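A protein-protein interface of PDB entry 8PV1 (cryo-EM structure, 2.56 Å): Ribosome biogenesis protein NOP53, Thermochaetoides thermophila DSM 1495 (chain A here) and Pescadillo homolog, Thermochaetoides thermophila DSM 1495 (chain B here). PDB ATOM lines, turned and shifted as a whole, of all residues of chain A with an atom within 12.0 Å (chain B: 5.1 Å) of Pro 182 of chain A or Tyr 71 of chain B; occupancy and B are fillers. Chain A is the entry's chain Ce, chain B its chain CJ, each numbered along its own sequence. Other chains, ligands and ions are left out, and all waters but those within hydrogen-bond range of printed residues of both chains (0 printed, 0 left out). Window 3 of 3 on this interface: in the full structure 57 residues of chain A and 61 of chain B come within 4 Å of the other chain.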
ATOM      1  N   PRO A 180      -0.410  12.767   8.212  1.00  0.00           N
ATOM      2  CA  PRO A 180      -0.563  13.449   6.922  1.00  0.00           C
ATOM      3  C   PRO A 180      -0.088  12.598   5.747  1.00  0.00           C
ATOM      4  O   PRO A 180       1.039  12.102   5.750  1.00  0.00           O
ATOM      5  CB  PRO A 180       0.302  14.702   7.080  1.00  0.00           C
ATOM      6  CG  PRO A 180       1.294  14.360   8.130  1.00  0.00           C
ATOM      7  CD  PRO A 180       0.640  13.373   9.048  1.00  0.00           C
ATOM      8  N   ASP A 181      -0.957  12.428   4.754  1.00  0.00           N
ATOM      9  CA  ASP A 181      -0.625  11.607   3.604  1.00  0.00           C
ATOM     10  C   ASP A 181       0.317  12.352   2.659  1.00  0.00           C
ATOM     11  O   ASP A 181       0.190  13.565   2.469  1.00  0.00           O
ATOM     12  CB  ASP A 181      -1.894  11.201   2.857  1.00  0.00           C
ATOM     13  CG  ASP A 181      -2.757  10.243   3.652  1.00  0.00           C
ATOM     14  OD1 ASP A 181      -2.416   9.965   4.821  1.00  0.00           O
ATOM     15  OD2 ASP A 181      -3.773   9.765   3.107  1.00  0.00           O
ATOM     16  N   PRO A 182       1.280  11.647   2.057  1.00  0.00           N
ATOM     17  CA  PRO A 182       2.152  12.248   1.031  1.00  0.00           C
ATOM     18  C   PRO A 182       1.501  12.225  -0.351  1.00  0.00           C
ATOM     19  O   PRO A 182       1.666  11.300  -1.151  1.00  0.00           O
ATOM     20  CB  PRO A 182       3.403  11.370   1.095  1.00  0.00           C
ATOM     21  CG  PRO A 182       2.941  10.052   1.659  1.00  0.00           C
ATOM     22  CD  PRO A 182       1.545  10.209   2.205  1.00  0.00           C
ATOM     23  N   LEU A 183       0.707  13.264  -0.630  1.00  0.00           N
ATOM     24  CA  LEU A 183       0.068  13.388  -1.937  1.00  0.00           C
ATOM     25  C   LEU A 183       1.090  13.565  -3.053  1.00  0.00           C
ATOM     26  O   LEU A 183       0.802  13.259  -4.216  1.00  0.00           O
ATOM     27  CB  LEU A 183      -0.918  14.557  -1.930  1.00  0.00           C
ATOM     28  CG  LEU A 183      -2.394  14.197  -1.738  1.00  0.00           C
ATOM     29  CD1 LEU A 183      -3.272  15.430  -1.875  1.00  0.00           C
ATOM     30  CD2 LEU A 183      -2.821  13.118  -2.722  1.00  0.00           C
ATOM     31  N   LYS A 184       2.283  14.053  -2.724  1.00  0.00           N
ATOM     32  CA  LYS A 184       3.389  14.119  -3.668  1.00  0.00           C
ATOM     33  C   LYS A 184       4.173  12.815  -3.582  1.00  0.00           C
ATOM     34  O   LYS A 184       4.566  12.395  -2.488  1.00  0.00           O
ATOM     35  CB  LYS A 184       4.300  15.314  -3.376  1.00  0.00           C
ATOM     36  CG  LYS A 184       3.641  16.690  -3.489  1.00  0.00           C
ATOM     37  CD  LYS A 184       3.049  17.164  -2.165  1.00  0.00           C
ATOM     38  CE  LYS A 184       2.333  18.494  -2.316  1.00  0.00           C
ATOM     39  NZ  LYS A 184       2.008  19.095  -0.993  1.00  0.00           N
ATOM     40  N   LYS A 185       4.380  12.171  -4.724  1.00  0.00           N
ATOM     41  CA  LYS A 185       5.171  10.950  -4.746  1.00  0.00           C
ATOM     42  C   LYS A 185       6.643  11.282  -4.509  1.00  0.00           C
ATOM     43  O   LYS A 185       7.111  12.351  -4.916  1.00  0.00           O
ATOM     44  CB  LYS A 185       5.010  10.226  -6.082  1.00  0.00           C
ATOM     45  CG  LYS A 185       3.623   9.673  -6.333  1.00  0.00           C
ATOM     46  CD  LYS A 185       3.523   9.053  -7.717  1.00  0.00           C
ATOM     47  CE  LYS A 185       4.594   7.997  -7.933  1.00  0.00           C
ATOM     48  NZ  LYS A 185       4.471   7.348  -9.267  1.00  0.00           N
ATOM     49  N   PRO A 186       7.393  10.403  -3.844  1.00  0.00           N
ATOM     50  CA  PRO A 186       8.834  10.632  -3.698  1.00  0.00           C
ATOM     51  C   PRO A 186       9.553  10.512  -5.032  1.00  0.00           C
ATOM     52  O   PRO A 186       9.113   9.807  -5.942  1.00  0.00           O
ATOM     53  CB  PRO A 186       9.273   9.532  -2.723  1.00  0.00           C
ATOM     54  CG  PRO A 186       8.017   9.083  -2.049  1.00  0.00           C
ATOM     55  CD  PRO A 186       6.940   9.237  -3.070  1.00  0.00           C
ATOM     56  N   LYS A 187      10.677  11.222  -5.141  1.00  0.00           N
ATOM     57  CA  LYS A 187      11.476  11.167  -6.361  1.00  0.00           C
ATOM     58  C   LYS A 187      12.236   9.850  -6.476  1.00  0.00           C
ATOM     59  O   LYS A 187      12.665   9.466  -7.575  1.00  0.00           O
ATOM     60  CB  LYS A 187      12.421  12.368  -6.400  1.00  0.00           C
ATOM     61  CG  LYS A 187      13.460  12.380  -5.296  1.00  0.00           C
ATOM     62  CD  LYS A 187      14.367  13.594  -5.411  1.00  0.00           C
ATOM     63  CE  LYS A 187      13.643  14.865  -5.000  1.00  0.00           C
ATOM     64  NZ  LYS A 187      14.555  16.042  -4.981  1.00  0.00           N
ATOM     65  N   THR A 188      12.389   9.133  -5.358  1.00  0.00           N
ATOM     66  CA  THR A 188      12.943   7.784  -5.404  1.00  0.00           C
ATOM     67  C   THR A 188      12.049   6.852  -6.211  1.00  0.00           C
ATOM     68  O   THR A 188      12.535   5.918  -6.859  1.00  0.00           O
ATOM     69  CB  THR A 188      13.136   7.248  -3.985  1.00  0.00           C
ATOM     70  OG1 THR A 188      11.946   7.469  -3.219  1.00  0.00           O
ATOM     71  CG2 THR A 188      14.307   7.940  -3.307  1.00  0.00           C
ATOM     72  N   LEU A 189      10.736   7.091  -6.184  1.00  0.00           N
ATOM     73  CA  LEU A 189       9.824   6.380  -7.072  1.00  0.00           C
ATOM     74  C   LEU A 189       9.967   6.830  -8.519  1.00  0.00           C
ATOM     75  O   LEU A 189       9.720   6.031  -9.429  1.00  0.00           O
ATOM     76  CB  LEU A 189       8.380   6.577  -6.615  1.00  0.00           C
ATOM     77  CG  LEU A 189       7.863   5.637  -5.529  1.00  0.00           C
ATOM     78  CD1 LEU A 189       6.376   5.851  -5.325  1.00  0.00           C
ATOM     79  CD2 LEU A 189       8.153   4.192  -5.887  1.00  0.00           C
ATOM     80  N   GLU A 190      10.350   8.088  -8.752  1.00  0.00           N
ATOM     81  CA  GLU A 190      10.532   8.567 -10.117  1.00  0.00           C
ATOM     82  C   GLU A 190      11.822   8.042 -10.733  1.00  0.00           C
ATOM     83  O   GLU A 190      11.985   8.097 -11.958  1.00  0.00           O
ATOM     84  CB  GLU A 190      10.517  10.094 -10.147  1.00  0.00           C
ATOM     85  CG  GLU A 190       9.326  10.724  -9.446  1.00  0.00           C
ATOM     86  CD  GLU A 190       9.501  12.214  -9.224  1.00  0.00           C
ATOM     87  OE1 GLU A 190      10.595  12.736  -9.526  1.00  0.00           O
ATOM     88  OE2 GLU A 190       8.546  12.863  -8.748  1.00  0.00           O
ATOM     89  N   GLN A 191      12.756   7.577  -9.904  1.00  0.00           N
ATOM     90  CA  GLN A 191      13.973   6.955 -10.426  1.00  0.00           C
ATOM     91  C   GLN A 191      13.658   5.711 -11.253  1.00  0.00           C
ATOM     92  O   GLN A 191      12.717   4.967 -10.961  1.00  0.00           O
ATOM     93  CB  GLN A 191      14.933   6.586  -9.293  1.00  0.00           C
ATOM     94  CG  GLN A 191      15.239   7.709  -8.332  1.00  0.00           C
ATOM     95  CD  GLN A 191      16.296   8.651  -8.863  1.00  0.00           C
ATOM     96  OE1 GLN A 191      17.178   8.250  -9.623  1.00  0.00           O
ATOM     97  NE2 GLN A 191      16.208   9.917  -8.477  1.00  0.00           N
ATOM     98  N   LYS B  40       2.219  -1.142  -6.572  1.00  0.00           N
ATOM     99  CA  LYS B  40       2.617   0.247  -6.404  1.00  0.00           C
ATOM    100  C   LYS B  40       3.904   0.597  -7.134  1.00  0.00           C
ATOM    101  O   LYS B  40       4.321   1.757  -7.097  1.00  0.00           O
ATOM    102  CB  LYS B  40       2.765   0.576  -4.917  1.00  0.00           C
ATOM    103  CG  LYS B  40       1.484   0.414  -4.125  1.00  0.00           C
ATOM    104  CD  LYS B  40       0.652   1.677  -4.165  1.00  0.00           C
ATOM    105  CE  LYS B  40       1.347   2.816  -3.448  1.00  0.00           C
ATOM    106  NZ  LYS B  40       0.451   3.993  -3.303  1.00  0.00           N
ATOM    107  N   THR B  66      14.200   3.560   1.470  1.00  0.00           N
ATOM    108  CA  THR B  66      13.516   3.898   2.712  1.00  0.00           C
ATOM    109  C   THR B  66      12.331   4.816   2.454  1.00  0.00           C
ATOM    110  O   THR B  66      11.256   4.625   3.031  1.00  0.00           O
ATOM    111  CB  THR B  66      14.503   4.543   3.689  1.00  0.00           C
ATOM    112  OG1 THR B  66      15.551   3.616   3.995  1.00  0.00           O
ATOM    113  CG2 THR B  66      13.815   4.966   4.979  1.00  0.00           C
ATOM    114  N   LYS B  67      12.491   5.790   1.555  1.00  0.00           N
ATOM    115  CA  LYS B  67      11.379   6.670   1.211  1.00  0.00           C
ATOM    116  C   LYS B  67      10.276   5.929   0.464  1.00  0.00           C
ATOM    117  O   LYS B  67       9.099   6.276   0.604  1.00  0.00           O
ATOM    118  CB  LYS B  67      11.881   7.853   0.386  1.00  0.00           C
ATOM    119  CG  LYS B  67      12.942   8.678   1.089  1.00  0.00           C
ATOM    120  CD  LYS B  67      12.397   9.308   2.356  1.00  0.00           C
ATOM    121  CE  LYS B  67      13.482  10.042   3.122  1.00  0.00           C
ATOM    122  NZ  LYS B  67      13.932  11.266   2.405  1.00  0.00           N
ATOM    123  N   ASP B  68      10.626   4.905  -0.321  1.00  0.00           N
ATOM    124  CA  ASP B  68       9.603   4.084  -0.963  1.00  0.00           C
ATOM    125  C   ASP B  68       8.787   3.308   0.066  1.00  0.00           C
ATOM    126  O   ASP B  68       7.559   3.205  -0.051  1.00  0.00           O
ATOM    127  CB  ASP B  68      10.247   3.130  -1.968  1.00  0.00           C
ATOM    128  CG  ASP B  68      10.685   3.832  -3.233  1.00  0.00           C
ATOM    129  OD1 ASP B  68      10.397   5.038  -3.370  1.00  0.00           O
ATOM    130  OD2 ASP B  68      11.311   3.178  -4.093  1.00  0.00           O
ATOM    131  N   ILE B  69       9.449   2.768   1.092  1.00  0.00           N
ATOM    132  CA  ILE B  69       8.713   2.086   2.156  1.00  0.00           C
ATOM    133  C   ILE B  69       7.882   3.083   2.965  1.00  0.00           C
ATOM    134  O   ILE B  69       6.767   2.771   3.412  1.00  0.00           O
ATOM    135  CB  ILE B  69       9.687   1.284   3.039  1.00  0.00           C
ATOM    136  CG1 ILE B  69      10.566   0.385   2.166  1.00  0.00           C
ATOM    137  CG2 ILE B  69       8.937   0.438   4.051  1.00  0.00           C
ATOM    138  CD1 ILE B  69       9.790  -0.578   1.294  1.00  0.00           C
ATOM    139  N   GLN B  70       8.400   4.302   3.150  1.00  0.00           N
ATOM    140  CA  GLN B  70       7.634   5.359   3.807  1.00  0.00           C
ATOM    141  C   GLN B  70       6.377   5.702   3.020  1.00  0.00           C
ATOM    142  O   GLN B  70       5.321   5.971   3.605  1.00  0.00           O
ATOM    143  CB  GLN B  70       8.492   6.611   3.981  1.00  0.00           C
ATOM    144  CG  GLN B  70       9.596   6.490   5.004  1.00  0.00           C
ATOM    145  CD  GLN B  70       9.089   6.008   6.332  1.00  0.00           C
ATOM    146  OE1 GLN B  70       9.517   4.970   6.832  1.00  0.00           O
ATOM    147  NE2 GLN B  70       8.156   6.750   6.909  1.00  0.00           N
ATOM    148  N   TYR B  71       6.482   5.724   1.692  1.00  0.00           N
ATOM    149  CA  TYR B  71       5.311   5.952   0.853  1.00  0.00           C
ATOM    150  C   TYR B  71       4.333   4.787   0.950  1.00  0.00           C
ATOM    151  O   TYR B  71       3.113   4.989   0.943  1.00  0.00           O
ATOM    152  CB  TYR B  71       5.745   6.173  -0.593  1.00  0.00           C
ATOM    153  CG  TYR B  71       4.618   6.556  -1.517  1.00  0.00           C
ATOM    154  CD1 TYR B  71       4.022   7.806  -1.429  1.00  0.00           C
ATOM    155  CD2 TYR B  71       4.151   5.671  -2.478  1.00  0.00           C
ATOM    156  CE1 TYR B  71       2.995   8.165  -2.272  1.00  0.00           C
ATOM    157  CE2 TYR B  71       3.122   6.022  -3.327  1.00  0.00           C
ATOM    158  CZ  TYR B  71       2.549   7.270  -3.218  1.00  0.00           C
ATOM    159  OH  TYR B  71       1.522   7.629  -4.059  1.00  0.00           O
ATOM    160  N   LEU B  72       4.853   3.559   1.036  1.00  0.00           N
ATOM    161  CA  LEU B  72       3.985   2.393   1.188  1.00  0.00           C
ATOM    162  C   LEU B  72       3.274   2.373   2.535  1.00  0.00           C
ATOM    163  O   LEU B  72       2.248   1.699   2.680  1.00  0.00           O
ATOM    164  CB  LEU B  72       4.784   1.103   1.019  1.00  0.00           C
ATOM    165  CG  LEU B  72       5.170   0.677  -0.393  1.00  0.00           C
ATOM    166  CD1 LEU B  72       5.835  -0.683  -0.342  1.00  0.00           C
ATOM    167  CD2 LEU B  72       3.948   0.650  -1.285  1.00  0.00           C
ATOM    168  N   LEU B  73       3.820   3.070   3.536  1.00  0.00           N
ATOM    169  CA  LEU B  73       3.162   3.147   4.841  1.00  0.00           C
ATOM    170  C   LEU B  73       1.784   3.800   4.785  1.00  0.00           C
ATOM    171  O   LEU B  73       0.941   3.506   5.639  1.00  0.00           O
ATOM    172  CB  LEU B  73       4.026   3.918   5.837  1.00  0.00           C
ATOM    173  CG  LEU B  73       5.045   3.136   6.658  1.00  0.00           C
ATOM    174  CD1 LEU B  73       6.014   4.096   7.316  1.00  0.00           C
ATOM    175  CD2 LEU B  73       4.339   2.288   7.696  1.00  0.00           C
ATOM    176  N   HIS B  74       1.534   4.676   3.816  1.00  0.00           N
ATOM    177  CA  HIS B  74       0.279   5.412   3.740  1.00  0.00           C
ATOM    178  C   HIS B  74      -0.700   4.837   2.726  1.00  0.00           C
ATOM    179  O   HIS B  74      -1.681   5.506   2.392  1.00  0.00           O
ATOM    180  CB  HIS B  74       0.551   6.880   3.408  1.00  0.00           C
ATOM    181  CG  HIS B  74       1.362   7.592   4.444  1.00  0.00           C
ATOM    182  ND1 HIS B  74       0.796   8.204   5.541  1.00  0.00           N
ATOM    183  CD2 HIS B  74       2.696   7.797   4.544  1.00  0.00           C
ATOM    184  CE1 HIS B  74       1.747   8.750   6.277  1.00  0.00           C
ATOM    185  NE2 HIS B  74       2.909   8.517   5.695  1.00  0.00           N
ATOM    186  N   GLU B  75      -0.460   3.634   2.230  1.00  0.00           N
ATOM    187  CA  GLU B  75      -1.336   3.058   1.217  1.00  0.00           C
ATOM    188  C   GLU B  75      -2.625   2.556   1.858  1.00  0.00           C
ATOM    189  O   GLU B  75      -2.573   1.818   2.848  1.00  0.00           O
ATOM    190  CB  GLU B  75      -0.621   1.925   0.484  1.00  0.00           C
ATOM    191  CG  GLU B  75      -1.527   1.033  -0.347  1.00  0.00           C
ATOM    192  CD  GLU B  75      -2.225   1.775  -1.472  1.00  0.00           C
ATOM    193  OE1 GLU B  75      -1.627   2.712  -2.037  1.00  0.00           O
ATOM    194  OE2 GLU B  75      -3.379   1.423  -1.791  1.00  0.00           O
ATOM    195  N   GLU B 129      -2.456   6.919  -9.856  1.00  0.00           N
ATOM    196  CA  GLU B 129      -1.150   7.225  -9.283  1.00  0.00           C
ATOM    197  C   GLU B 129      -0.020   6.699 -10.161  1.00  0.00           C
ATOM    198  O   GLU B 129       0.979   7.394 -10.383  1.00  0.00           O
ATOM    199  CB  GLU B 129      -1.056   6.637  -7.874  1.00  0.00           C
ATOM    200  CG  GLU B 129       0.356   6.521  -7.333  1.00  0.00           C
ATOM    201  CD  GLU B 129       0.454   5.547  -6.180  1.00  0.00           C
ATOM    202  OE1 GLU B 129      -0.526   5.428  -5.416  1.00  0.00           O
ATOM    203  OE2 GLU B 129       1.512   4.897  -6.042  1.00  0.00           O
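Of the 12 printed residues of chain B, 5 touch a printed residue of chain A. Among the printed residues, 11 pairs touch across the chains.
Pro 180 of chain A touches His 74 of chain B (O to CE1, 3.5 Å). His 74 of chain B touches Asp 181 of chain A (ND1 to OD1, 3.7 Å). CE1 of Tyr 71 of chain B touches O of Pro 182 of chain A, 3.6 Å away. Pro 182 of chain A touches His 74 of chain B. Tyr 71 of chain B touches Lys 185 of chain A. NZ of Lys 185 of chain A touches O of Glu 129 of chain B (3.7 Å). Tyr 71 of chain B touches Pro 186 of chain A (CD1 to CD, 3.6 Å). Thr 188 of chain A touches Lys 67 of chain B. Leu 189 of chain A touches Tyr 71 of chain B (CD1 to CD2, 3.6 Å).
NZ of Lys 40 of chain B lies within salt-bridge range of OE1 of Glu 129 of chain B, 2.7 Å away. The side-chain hydroxyl (OH) of Tyr 71 of chain B sits close to the side-chain carboxylate (OE1) of Glu 129 of chain B (3.3 Å).
Pro 182 of chain A touches just these residues of chain B: Tyr 71 (3.6 Å) and His 74 (3.4 Å). Tyr 71 of chain B touches just these residues of chain A: Pro 182, Lys 185, Pro 186 and Leu 189. No residue of chain A comes within 4 Å of Gln 70 of chain B. No residue of chain A comes within 4 Å of Leu 73 of chain B. No residue of chain A comes within 4 Å of Glu 75 of chain B. Printed residues of chain A within 4 Å of Lys 67 of chain B: Thr 188 (3.6 Å). Of the printed residues of chain B, Lys 185 of chain A touches Tyr 71 and Glu 129. Of the printed residues of chain B, Asp 181 of chain A touches His 74. Gln 191 of chain A touches none of the printed residues of chain B. The nearest printed residue of chain B that does not touch Pro 182 of chain A is Gln 70 of chain B (5.1 Å). The nearest printed residue of chain B that does not touch Leu 189 of chain A is Lys 40 of chain B (4.7 Å).
The side-chain carboxylate (OD1) of Asp 68 of chain B sits close to the backbone NH (N) of Leu 189 of chain A (3.5 Å). The side-chain carboxylate of Asp 68 of chain B lies within hydrogen-bond range of the side-chain hydroxyl of Thr 188 of chain A (2.9 Å).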
